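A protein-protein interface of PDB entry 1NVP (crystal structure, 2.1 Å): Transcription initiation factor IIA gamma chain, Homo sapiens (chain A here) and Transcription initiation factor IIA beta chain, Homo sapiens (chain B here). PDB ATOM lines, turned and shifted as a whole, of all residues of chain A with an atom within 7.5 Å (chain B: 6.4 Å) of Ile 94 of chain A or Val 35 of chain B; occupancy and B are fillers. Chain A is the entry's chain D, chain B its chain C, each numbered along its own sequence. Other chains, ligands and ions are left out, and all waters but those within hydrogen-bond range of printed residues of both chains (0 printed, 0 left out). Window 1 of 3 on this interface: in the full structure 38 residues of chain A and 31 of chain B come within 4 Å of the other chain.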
ATOM      1  N   LEU A   4     -15.483  -7.495   0.735  1.00  0.00           N
ATOM      2  CA  LEU A   4     -16.174  -6.225   0.827  1.00  0.00           C
ATOM      3  C   LEU A   4     -15.822  -5.217  -0.263  1.00  0.00           C
ATOM      4  O   LEU A   4     -16.705  -4.615  -0.876  1.00  0.00           O
ATOM      5  CB  LEU A   4     -15.854  -5.618   2.196  1.00  0.00           C
ATOM      6  CG  LEU A   4     -16.508  -4.327   2.678  1.00  0.00           C
ATOM      7  CD1 LEU A   4     -17.980  -4.571   2.967  1.00  0.00           C
ATOM      8  CD2 LEU A   4     -15.797  -3.848   3.929  1.00  0.00           C
ATOM      9  N   ASN A   7     -16.618  -4.586  -5.131  1.00  0.00           N
ATOM     10  CA  ASN A   7     -17.454  -3.731  -5.967  1.00  0.00           C
ATOM     11  C   ASN A   7     -17.126  -2.274  -5.698  1.00  0.00           C
ATOM     12  O   ASN A   7     -17.939  -1.515  -5.169  1.00  0.00           O
ATOM     13  CB  ASN A   7     -18.945  -3.956  -5.730  1.00  0.00           C
ATOM     14  CG  ASN A   7     -19.800  -3.268  -6.786  1.00  0.00           C
ATOM     15  OD1 ASN A   7     -19.998  -3.795  -7.883  1.00  0.00           O
ATOM     16  ND2 ASN A   7     -20.288  -2.073  -6.468  1.00  0.00           N
ATOM     17  N   THR A   8     -15.903  -1.914  -6.054  1.00  0.00           N
ATOM     18  CA  THR A   8     -15.389  -0.561  -5.921  1.00  0.00           C
ATOM     19  C   THR A   8     -14.780  -0.323  -7.295  1.00  0.00           C
ATOM     20  O   THR A   8     -14.706  -1.252  -8.102  1.00  0.00           O
ATOM     21  CB  THR A   8     -14.279  -0.479  -4.854  1.00  0.00           C
ATOM     22  OG1 THR A   8     -13.266  -1.450  -5.147  1.00  0.00           O
ATOM     23  CG2 THR A   8     -14.842  -0.749  -3.470  1.00  0.00           C
ATOM     24  N   PHE A  57     -20.850  12.777   7.666  1.00  0.00           N
ATOM     25  CA  PHE A  57     -21.980  12.872   6.754  1.00  0.00           C
ATOM     26  C   PHE A  57     -23.322  12.967   7.462  1.00  0.00           C
ATOM     27  O   PHE A  57     -23.509  12.433   8.553  1.00  0.00           O
ATOM     28  CB  PHE A  57     -21.981  11.691   5.772  1.00  0.00           C
ATOM     29  CG  PHE A  57     -22.251  10.353   6.407  1.00  0.00           C
ATOM     30  CD1 PHE A  57     -23.472   9.717   6.218  1.00  0.00           C
ATOM     31  CD2 PHE A  57     -21.270   9.708   7.154  1.00  0.00           C
ATOM     32  CE1 PHE A  57     -23.709   8.450   6.752  1.00  0.00           C
ATOM     33  CE2 PHE A  57     -21.498   8.442   7.693  1.00  0.00           C
ATOM     34  CZ  PHE A  57     -22.720   7.814   7.492  1.00  0.00           C
ATOM     35  N   LEU A  61     -32.343   9.046   6.359  1.00  0.00           N
ATOM     36  CA  LEU A  61     -32.269   7.615   6.128  1.00  0.00           C
ATOM     37  C   LEU A  61     -33.556   7.159   5.456  1.00  0.00           C
ATOM     38  O   LEU A  61     -34.652   7.365   5.977  1.00  0.00           O
ATOM     39  CB  LEU A  61     -32.063   6.876   7.454  1.00  0.00           C
ATOM     40  CG  LEU A  61     -31.834   5.366   7.365  1.00  0.00           C
ATOM     41  CD1 LEU A  61     -30.586   5.096   6.534  1.00  0.00           C
ATOM     42  CD2 LEU A  61     -31.684   4.774   8.768  1.00  0.00           C
ATOM     43  N   THR A  63     -33.768   3.780   3.947  1.00  0.00           N
ATOM     44  CA  THR A  63     -33.921   2.376   4.294  1.00  0.00           C
ATOM     45  C   THR A  63     -32.704   1.845   5.033  1.00  0.00           C
ATOM     46  O   THR A  63     -31.619   2.424   4.981  1.00  0.00           O
ATOM     47  CB  THR A  63     -34.122   1.490   3.050  1.00  0.00           C
ATOM     48  OG1 THR A  63     -32.980   1.607   2.191  1.00  0.00           O
ATOM     49  CG2 THR A  63     -35.365   1.900   2.294  1.00  0.00           C
ATOM     50  N   ARG A  65     -31.131  -2.194   6.577  1.00  0.00           N
ATOM     51  CA  ARG A  65     -31.294  -3.631   6.600  1.00  0.00           C
ATOM     52  C   ARG A  65     -30.106  -4.176   7.351  1.00  0.00           C
ATOM     53  O   ARG A  65     -29.010  -3.613   7.299  1.00  0.00           O
ATOM     54  CB  ARG A  65     -31.324  -4.232   5.197  1.00  0.00           C
ATOM     55  CG  ARG A  65     -31.346  -5.749   5.229  1.00  0.00           C
ATOM     56  CD  ARG A  65     -31.175  -6.411   3.864  1.00  0.00           C
ATOM     57  NE  ARG A  65     -32.366  -6.335   3.020  1.00  0.00           N
ATOM     58  CZ  ARG A  65     -32.672  -5.300   2.247  1.00  0.00           C
ATOM     59  NH1 ARG A  65     -31.872  -4.244   2.206  1.00  0.00           N
ATOM     60  NH2 ARG A  65     -33.769  -5.323   1.509  1.00  0.00           N
ATOM     61  N   VAL A  70     -24.416  -7.756   8.448  1.00  0.00           N
ATOM     62  CA  VAL A  70     -24.051  -6.744   7.467  1.00  0.00           C
ATOM     63  C   VAL A  70     -25.136  -5.679   7.335  1.00  0.00           C
ATOM     64  O   VAL A  70     -26.282  -5.987   7.018  1.00  0.00           O
ATOM     65  CB  VAL A  70     -23.826  -7.373   6.074  1.00  0.00           C
ATOM     66  CG1 VAL A  70     -23.742  -6.279   5.011  1.00  0.00           C
ATOM     67  CG2 VAL A  70     -22.550  -8.198   6.081  1.00  0.00           C
ATOM     68  N   TRP A  71     -24.767  -4.427   7.573  1.00  0.00           N
ATOM     69  CA  TRP A  71     -25.707  -3.320   7.448  1.00  0.00           C
ATOM     70  C   TRP A  71     -25.688  -2.726   6.041  1.00  0.00           C
ATOM     71  O   TRP A  71     -24.621  -2.493   5.465  1.00  0.00           O
ATOM     72  CB  TRP A  71     -25.378  -2.199   8.437  1.00  0.00           C
ATOM     73  CG  TRP A  71     -25.782  -2.459   9.855  1.00  0.00           C
ATOM     74  CD1 TRP A  71     -24.989  -2.932  10.859  1.00  0.00           C
ATOM     75  CD2 TRP A  71     -27.067  -2.207  10.441  1.00  0.00           C
ATOM     76  NE1 TRP A  71     -25.697  -2.981  12.041  1.00  0.00           N
ATOM     77  CE2 TRP A  71     -26.976  -2.541  11.812  1.00  0.00           C
ATOM     78  CE3 TRP A  71     -28.286  -1.727   9.942  1.00  0.00           C
ATOM     79  CZ2 TRP A  71     -28.060  -2.412  12.696  1.00  0.00           C
ATOM     80  CZ3 TRP A  71     -29.371  -1.597  10.824  1.00  0.00           C
ATOM     81  CH2 TRP A  71     -29.244  -1.938  12.185  1.00  0.00           C
ATOM     82  N   THR A  72     -26.875  -2.484   5.500  1.00  0.00           N
ATOM     83  CA  THR A  72     -27.040  -1.879   4.184  1.00  0.00           C
ATOM     84  C   THR A  72     -28.010  -0.707   4.338  1.00  0.00           C
ATOM     85  O   THR A  72     -29.193  -0.908   4.633  1.00  0.00           O
ATOM     86  CB  THR A  72     -27.652  -2.860   3.171  1.00  0.00           C
ATOM     87  OG1 THR A  72     -26.796  -3.996   3.017  1.00  0.00           O
ATOM     88  CG2 THR A  72     -27.836  -2.181   1.818  1.00  0.00           C
ATOM     89  N   PHE A  73     -27.511   0.511   4.157  1.00  0.00           N
ATOM     90  CA  PHE A  73     -28.348   1.698   4.261  1.00  0.00           C
ATOM     91  C   PHE A  73     -28.491   2.377   2.906  1.00  0.00           C
ATOM     92  O   PHE A  73     -27.803   2.037   1.943  1.00  0.00           O
ATOM     93  CB  PHE A  73     -27.744   2.726   5.217  1.00  0.00           C
ATOM     94  CG  PHE A  73     -27.400   2.185   6.568  1.00  0.00           C
ATOM     95  CD1 PHE A  73     -26.076   1.939   6.913  1.00  0.00           C
ATOM     96  CD2 PHE A  73     -28.394   1.960   7.515  1.00  0.00           C
ATOM     97  CE1 PHE A  73     -25.744   1.477   8.179  1.00  0.00           C
ATOM     98  CE2 PHE A  73     -28.074   1.497   8.784  1.00  0.00           C
ATOM     99  CZ  PHE A  73     -26.746   1.257   9.121  1.00  0.00           C
ATOM    100  N   VAL A  74     -29.400   3.342   2.852  1.00  0.00           N
ATOM    101  CA  VAL A  74     -29.640   4.145   1.664  1.00  0.00           C
ATOM    102  C   VAL A  74     -30.077   5.491   2.218  1.00  0.00           C
ATOM    103  O   VAL A  74     -31.156   5.603   2.811  1.00  0.00           O
ATOM    104  CB  VAL A  74     -30.760   3.584   0.782  1.00  0.00           C
ATOM    105  CG1 VAL A  74     -31.052   4.558  -0.350  1.00  0.00           C
ATOM    106  CG2 VAL A  74     -30.366   2.244   0.219  1.00  0.00           C
ATOM    107  N   LEU A  75     -29.214   6.492   2.066  1.00  0.00           N
ATOM    108  CA  LEU A  75     -29.484   7.845   2.540  1.00  0.00           C
ATOM    109  C   LEU A  75     -29.869   8.730   1.355  1.00  0.00           C
ATOM    110  O   LEU A  75     -29.464   8.466   0.223  1.00  0.00           O
ATOM    111  CB  LEU A  75     -28.239   8.437   3.198  1.00  0.00           C
ATOM    112  CG  LEU A  75     -27.665   7.932   4.523  1.00  0.00           C
ATOM    113  CD1 LEU A  75     -28.429   8.549   5.665  1.00  0.00           C
ATOM    114  CD2 LEU A  75     -27.701   6.417   4.581  1.00  0.00           C
ATOM    115  N   VAL A  78     -27.688  13.630   1.054  1.00  0.00           N
ATOM    116  CA  VAL A  78     -26.572  13.549   1.989  1.00  0.00           C
ATOM    117  C   VAL A  78     -25.502  14.609   1.756  1.00  0.00           C
ATOM    118  O   VAL A  78     -25.364  15.149   0.658  1.00  0.00           O
ATOM    119  CB  VAL A  78     -25.896  12.172   1.905  1.00  0.00           C
ATOM    120  CG1 VAL A  78     -24.983  11.967   3.102  1.00  0.00           C
ATOM    121  CG2 VAL A  78     -26.949  11.089   1.820  1.00  0.00           C
ATOM    122  N   PHE A  80     -21.493  14.820   2.573  1.00  0.00           N
ATOM    123  CA  PHE A  80     -20.253  14.260   3.081  1.00  0.00           C
ATOM    124  C   PHE A  80     -19.276  15.387   3.354  1.00  0.00           C
ATOM    125  O   PHE A  80     -18.954  16.185   2.473  1.00  0.00           O
ATOM    126  CB  PHE A  80     -19.682  13.249   2.091  1.00  0.00           C
ATOM    127  CG  PHE A  80     -20.520  12.012   1.966  1.00  0.00           C
ATOM    128  CD1 PHE A  80     -21.620  11.980   1.114  1.00  0.00           C
ATOM    129  CD2 PHE A  80     -20.231  10.887   2.727  1.00  0.00           C
ATOM    130  CE1 PHE A  80     -22.428  10.849   1.036  1.00  0.00           C
ATOM    131  CE2 PHE A  80     -21.032   9.755   2.657  1.00  0.00           C
ATOM    132  CZ  PHE A  80     -22.130   9.732   1.804  1.00  0.00           C
ATOM    133  N   VAL A  92     -27.206   7.797  -1.671  1.00  0.00           N
ATOM    134  CA  VAL A  92     -25.993   7.031  -1.421  1.00  0.00           C
ATOM    135  C   VAL A  92     -26.342   5.721  -0.722  1.00  0.00           C
ATOM    136  O   VAL A  92     -27.156   5.693   0.201  1.00  0.00           O
ATOM    137  CB  VAL A  92     -24.999   7.822  -0.541  1.00  0.00           C
ATOM    138  CG1 VAL A  92     -25.622   8.131   0.804  1.00  0.00           C
ATOM    139  CG2 VAL A  92     -23.715   7.026  -0.361  1.00  0.00           C
ATOM    140  N   LYS A  93     -25.728   4.636  -1.180  1.00  0.00           N
ATOM    141  CA  LYS A  93     -25.956   3.311  -0.619  1.00  0.00           C
ATOM    142  C   LYS A  93     -24.721   2.919   0.186  1.00  0.00           C
ATOM    143  O   LYS A  93     -23.595   2.996  -0.314  1.00  0.00           O
ATOM    144  CB  LYS A  93     -26.187   2.313  -1.749  1.00  0.00           C
ATOM    145  CG  LYS A  93     -26.527   0.907  -1.314  1.00  0.00           C
ATOM    146  CD  LYS A  93     -26.249  -0.050  -2.458  1.00  0.00           C
ATOM    147  CE  LYS A  93     -26.812  -1.430  -2.200  1.00  0.00           C
ATOM    148  NZ  LYS A  93     -28.282  -1.465  -2.428  1.00  0.00           N
ATOM    149  N   ILE A  94     -24.928   2.507   1.431  1.00  0.00           N
ATOM    150  CA  ILE A  94     -23.819   2.127   2.297  1.00  0.00           C
ATOM    151  C   ILE A  94     -23.900   0.682   2.755  1.00  0.00           C
ATOM    152  O   ILE A  94     -24.864   0.285   3.411  1.00  0.00           O
ATOM    153  CB  ILE A  94     -23.761   3.010   3.563  1.00  0.00           C
ATOM    154  CG1 ILE A  94     -23.625   4.483   3.178  1.00  0.00           C
ATOM    155  CG2 ILE A  94     -22.584   2.594   4.434  1.00  0.00           C
ATOM    156  CD1 ILE A  94     -23.612   5.434   4.370  1.00  0.00           C
ATOM    157  N   VAL A  95     -22.891  -0.105   2.398  1.00  0.00           N
ATOM    158  CA  VAL A  95     -22.831  -1.499   2.813  1.00  0.00           C
ATOM    159  C   VAL A  95     -21.696  -1.561   3.823  1.00  0.00           C
ATOM    160  O   VAL A  95     -20.585  -1.109   3.544  1.00  0.00           O
ATOM    161  CB  VAL A  95     -22.525  -2.433   1.638  1.00  0.00           C
ATOM    162  CG1 VAL A  95     -22.531  -3.878   2.113  1.00  0.00           C
ATOM    163  CG2 VAL A  95     -23.558  -2.241   0.550  1.00  0.00           C
ATOM    164  N   ALA A  96     -21.977  -2.103   5.002  1.00  0.00           N
ATOM    165  CA  ALA A  96     -20.966  -2.171   6.045  1.00  0.00           C
ATOM    166  C   ALA A  96     -20.894  -3.510   6.767  1.00  0.00           C
ATOM    167  O   ALA A  96     -21.894  -3.995   7.306  1.00  0.00           O
ATOM    168  CB  ALA A  96     -21.205  -1.046   7.061  1.00  0.00           C
ATOM    169  N   ASN B  33     -23.712   6.283  -6.277  1.00  0.00           N
ATOM    170  CA  ASN B  33     -22.963   6.679  -5.112  1.00  0.00           C
ATOM    171  C   ASN B  33     -23.003   5.498  -4.144  1.00  0.00           C
ATOM    172  O   ASN B  33     -24.072   5.030  -3.736  1.00  0.00           O
ATOM    173  CB  ASN B  33     -23.614   7.925  -4.547  1.00  0.00           C
ATOM    174  CG  ASN B  33     -23.907   8.943  -5.631  1.00  0.00           C
ATOM    175  OD1 ASN B  33     -22.997   9.578  -6.162  1.00  0.00           O
ATOM    176  ND2 ASN B  33     -25.176   9.078  -5.988  1.00  0.00           N
ATOM    177  N   VAL B  34     -21.827   4.986  -3.809  1.00  0.00           N
ATOM    178  CA  VAL B  34     -21.744   3.849  -2.915  1.00  0.00           C
ATOM    179  C   VAL B  34     -20.610   3.999  -1.928  1.00  0.00           C
ATOM    180  O   VAL B  34     -19.599   4.647  -2.203  1.00  0.00           O
ATOM    181  CB  VAL B  34     -21.527   2.535  -3.696  1.00  0.00           C
ATOM    182  CG1 VAL B  34     -21.368   1.366  -2.730  1.00  0.00           C
ATOM    183  CG2 VAL B  34     -22.689   2.285  -4.630  1.00  0.00           C
ATOM    184  N   VAL B  35     -20.800   3.400  -0.764  1.00  0.00           N
ATOM    185  CA  VAL B  35     -19.794   3.404   0.273  1.00  0.00           C
ATOM    186  C   VAL B  35     -19.715   1.965   0.736  1.00  0.00           C
ATOM    187  O   VAL B  35     -20.729   1.348   1.066  1.00  0.00           O
ATOM    188  CB  VAL B  35     -20.187   4.293   1.463  1.00  0.00           C
ATOM    189  CG1 VAL B  35     -19.192   4.110   2.602  1.00  0.00           C
ATOM    190  CG2 VAL B  35     -20.232   5.741   1.033  1.00  0.00           C
ATOM    191  N   VAL B  36     -18.512   1.412   0.707  1.00  0.00           N
ATOM    192  CA  VAL B  36     -18.309   0.051   1.155  1.00  0.00           C
ATOM    193  C   VAL B  36     -17.314   0.200   2.281  1.00  0.00           C
ATOM    194  O   VAL B  36     -16.232   0.760   2.103  1.00  0.00           O
ATOM    195  CB  VAL B  36     -17.763  -0.835   0.035  1.00  0.00           C
ATOM    196  CG1 VAL B  36     -17.510  -2.222   0.561  1.00  0.00           C
ATOM    197  CG2 VAL B  36     -18.773  -0.901  -1.101  1.00  0.00           C
ATOM    198  N   CYS B  37     -17.705  -0.268   3.458  1.00  0.00           N
ATOM    199  CA  CYS B  37     -16.864  -0.134   4.629  1.00  0.00           C
ATOM    200  C   CYS B  37     -17.216  -1.168   5.675  1.00  0.00           C
ATOM    201  O   CYS B  37     -17.900  -2.157   5.406  1.00  0.00           O
ATOM    202  CB  CYS B  37     -17.055   1.256   5.240  1.00  0.00           C
ATOM    203  SG  CYS B  37     -18.774   1.568   5.781  1.00  0.00           S
ATOM    204  N   PHE B  51     -24.102   6.781  12.762  1.00  0.00           N
ATOM    205  CA  PHE B  51     -23.232   5.750  12.221  1.00  0.00           C
ATOM    206  C   PHE B  51     -21.763   6.012  12.520  1.00  0.00           C
ATOM    207  O   PHE B  51     -21.261   7.118  12.320  1.00  0.00           O
ATOM    208  CB  PHE B  51     -23.416   5.636  10.705  1.00  0.00           C
ATOM    209  CG  PHE B  51     -24.843   5.769  10.246  1.00  0.00           C
ATOM    210  CD1 PHE B  51     -25.480   7.008  10.254  1.00  0.00           C
ATOM    211  CD2 PHE B  51     -25.543   4.660   9.784  1.00  0.00           C
ATOM    212  CE1 PHE B  51     -26.793   7.140   9.802  1.00  0.00           C
ATOM    213  CE2 PHE B  51     -26.854   4.781   9.329  1.00  0.00           C
ATOM    214  CZ  PHE B  51     -27.481   6.024   9.339  1.00  0.00           C
ATOM    215  N   LEU B  53     -18.475   4.575  11.257  1.00  0.00           N
ATOM    216  CA  LEU B  53     -17.836   3.741  10.241  1.00  0.00           C
ATOM    217  C   LEU B  53     -16.318   3.916  10.099  1.00  0.00           C
ATOM    218  O   LEU B  53     -15.742   4.903  10.567  1.00  0.00           O
ATOM    219  CB  LEU B  53     -18.515   4.010   8.897  1.00  0.00           C
ATOM    220  CG  LEU B  53     -20.046   4.038   8.962  1.00  0.00           C
ATOM    221  CD1 LEU B  53     -20.627   4.474   7.628  1.00  0.00           C
ATOM    222  CD2 LEU B  53     -20.556   2.662   9.338  1.00  0.00           C
ATOM    223  N   GLY B  56     -13.319   2.906   4.685  1.00  0.00           N
ATOM    224  CA  GLY B  56     -14.270   2.936   3.593  1.00  0.00           C
ATOM    225  C   GLY B  56     -13.797   3.537   2.284  1.00  0.00           C
ATOM    226  O   GLY B  56     -12.989   4.466   2.253  1.00  0.00           O
ATOM    227  N   ILE B  57     -14.310   2.982   1.193  1.00  0.00           N
ATOM    228  CA  ILE B  57     -13.996   3.455  -0.143  1.00  0.00           C
ATOM    229  C   ILE B  57     -15.303   3.977  -0.724  1.00  0.00           C
ATOM    230  O   ILE B  57     -16.261   3.221  -0.893  1.00  0.00           O
ATOM    231  CB  ILE B  57     -13.461   2.323  -1.043  1.00  0.00           C
ATOM    232  CG1 ILE B  57     -12.088   1.865  -0.540  1.00  0.00           C
ATOM    233  CG2 ILE B  57     -13.377   2.807  -2.482  1.00  0.00           C
ATOM    234  CD1 ILE B  57     -11.469   0.750  -1.363  1.00  0.00           C
ATOM    235  N   MET B  58     -15.339   5.268  -1.028  1.00  0.00           N
ATOM    236  CA  MET B  58     -16.544   5.879  -1.562  1.00  0.00           C
ATOM    237  C   MET B  58     -16.406   6.343  -3.001  1.00  0.00           C
ATOM    238  O   MET B  58     -15.334   6.757  -3.437  1.00  0.00           O
ATOM    239  CB  MET B  58     -16.943   7.092  -0.719  1.00  0.00           C
ATOM    240  CG  MET B  58     -16.874   6.892   0.783  1.00  0.00           C
ATOM    241  SD  MET B  58     -17.537   8.334   1.638  1.00  0.00           S
ATOM    242  CE  MET B  58     -16.064   9.154   2.202  1.00  0.00           C
ATOM    243  N   ASN B  59     -17.512   6.273  -3.728  1.00  0.00           N
ATOM    244  CA  ASN B  59     -17.565   6.740  -5.101  1.00  0.00           C
ATOM    245  C   ASN B  59     -18.782   7.656  -5.145  1.00  0.00           C
ATOM    246  O   ASN B  59     -19.916   7.202  -5.298  1.00  0.00           O
ATOM    247  CB  ASN B  59     -17.730   5.576  -6.078  1.00  0.00           C
ATOM    248  CG  ASN B  59     -17.691   6.031  -7.523  1.00  0.00           C
ATOM    249  OD1 ASN B  59     -18.726   6.179  -8.168  1.00  0.00           O
ATOM    250  ND2 ASN B  59     -16.491   6.275  -8.034  1.00  0.00           N
ATOM    251  N   LEU B  60     -18.529   8.950  -4.984  1.00  0.00           N
ATOM    252  CA  LEU B  60     -19.579   9.957  -4.963  1.00  0.00           C
ATOM    253  C   LEU B  60     -19.522  10.859  -6.194  1.00  0.00           C
ATOM    254  O   LEU B  60     -18.486  11.458  -6.490  1.00  0.00           O
ATOM    255  CB  LEU B  60     -19.433  10.805  -3.698  1.00  0.00           C
ATOM    256  CG  LEU B  60     -19.198  10.000  -2.416  1.00  0.00           C
ATOM    257  CD1 LEU B  60     -18.723  10.917  -1.305  1.00  0.00           C
ATOM    258  CD2 LEU B  60     -20.475   9.277  -2.027  1.00  0.00           C
ATOM    259  N   PHE B  67     -11.673   6.810   3.516  1.00  0.00           N
ATOM    260  CA  PHE B  67     -11.654   7.297   4.891  1.00  0.00           C
ATOM    261  C   PHE B  67     -11.271   6.183   5.849  1.00  0.00           C
ATOM    262  O   PHE B  67     -11.521   5.006   5.585  1.00  0.00           O
ATOM    263  CB  PHE B  67     -13.021   7.888   5.292  1.00  0.00           C
ATOM    264  CG  PHE B  67     -14.144   6.876   5.372  1.00  0.00           C
ATOM    265  CD1 PHE B  67     -14.158   5.896   6.363  1.00  0.00           C
ATOM    266  CD2 PHE B  67     -15.195   6.918   4.460  1.00  0.00           C
ATOM    267  CE1 PHE B  67     -15.198   4.975   6.443  1.00  0.00           C
ATOM    268  CE2 PHE B  67     -16.242   6.003   4.531  1.00  0.00           C
ATOM    269  CZ  PHE B  67     -16.243   5.028   5.525  1.00  0.00           C
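The backbone NH (N) of Lys 93 of chain A sits at hydrogen-bond distance from the backbone carbonyl oxygen (O) of Asn 33 of chain B (3.1 Å). O of Lys 93 of chain A is in hydrogen-bond range of N of Val 35 of chain B (2.9 Å). The backbone carbonyl oxygen (O) of Val 35 of chain B is in hydrogen-bond range of the backbone NH (N) of Val 95 of chain A (2.9 Å). O of Val 95 of chain A lies within hydrogen-bond range of N of Cys 37 of chain B (3.0 Å).
The backbone carbonyl oxygen of Val 34 of chain B sits at hydrogen-bond distance from the backbone NH of Asn 59 of chain B (3.1 Å). N of Ile 57 of chain B lies within hydrogen-bond range of O of Val 36 of chain B, 3.1 Å away. The backbone carbonyl oxygen (O) of Trp 71 of chain A sits at hydrogen-bond distance from the backbone NH (N) of Ala 96 of chain A, 2.7 Å away. O of Ile 94 of chain A lies within hydrogen-bond range of N of Phe 73 of chain A. N of Leu 75 of chain A lies within hydrogen-bond range of O of Val 92 of chain A (2.9 Å).
Among the printed residues, pairs that only touch across the chains: Leu 4 of chain A with Val 36 of chain B (2.9 Å), Leu 4 of chain A with Cys 37 of chain B (3.1 Å), Ala 96 of chain A with Cys 37 of chain B (3.1 Å), Lys 93 of chain A with Val 34 of chain B (3.3 Å), Ile 94 of chain A with Val 35 of chain B (3.4 Å), Val 95 of chain A with Val 36 of chain B (3.5 Å), Phe 73 of chain A with Phe 51 of chain B (3.5 Å), Val 92 of chain A with Asn 33 of chain B (3.6 Å), Phe 80 of chain A with Met 58 of chain B (3.9 Å), Phe 80 of chain A with Leu 60 of chain B (3.9 Å), Phe 57 of chain A with Phe 51 of chain B (3.9 Å), Phe 57 of chain A with Leu 53 of chain B (3.9 Å), Val 92 of chain A with Val 35 of chain B (3.97 Å) and Thr 8 of chain A with Ile 57 of chain B (3.97 Å).
Val 70 of chain A touches none of the printed residues of chain B. Of the printed residues of chain B, Phe 73 of chain A touches Phe 51. Of the printed residues of chain B, Phe 80 of chain A touches Met 58 and Leu 60. Of chain B, only Val 35 comes within 4 Å of Ile 94 of chain A. Val 35 of chain B touches just these residues of chain A: Val 92 (3.97 Å), Lys 93 (2.9 Å), Ile 94 (3.4 Å) and Val 95 (2.9 Å). Printed residues of chain A within 4 Å of Cys 37 of chain B: Leu 4 (3.1 Å), Val 95 (3.0 Å) and Ala 96 (3.1 Å). The nearest residue of chain A that does not touch Val 35 of chain B is Phe 80 of chain A (4.4 Å). The nearest printed residue of chain B that does not touch Leu 4 of chain A is Val 35 of chain B (6.8 Å).
Of the 20 printed residues of chain A, 10 touch a printed residue of chain B. Printed residues of chain A that touch a printed residue of chain B: Leu 4, Thr 8, Phe 57, Phe 73, Phe 80, Val 92, Lys 93, Ile 94, Val 95 and Ala 96. Hydrophobic or aromatic side chains of chain B that line the printed part of chain A: Val 34, Val 35, Val 36, Phe 51, Leu 53, Ile 57, Met 58 and Leu 60. Along chain B the printed residues that touch a printed residue of chain A span positions 33 to 60. Among the printed residues, 18 pairs touch across the chains.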
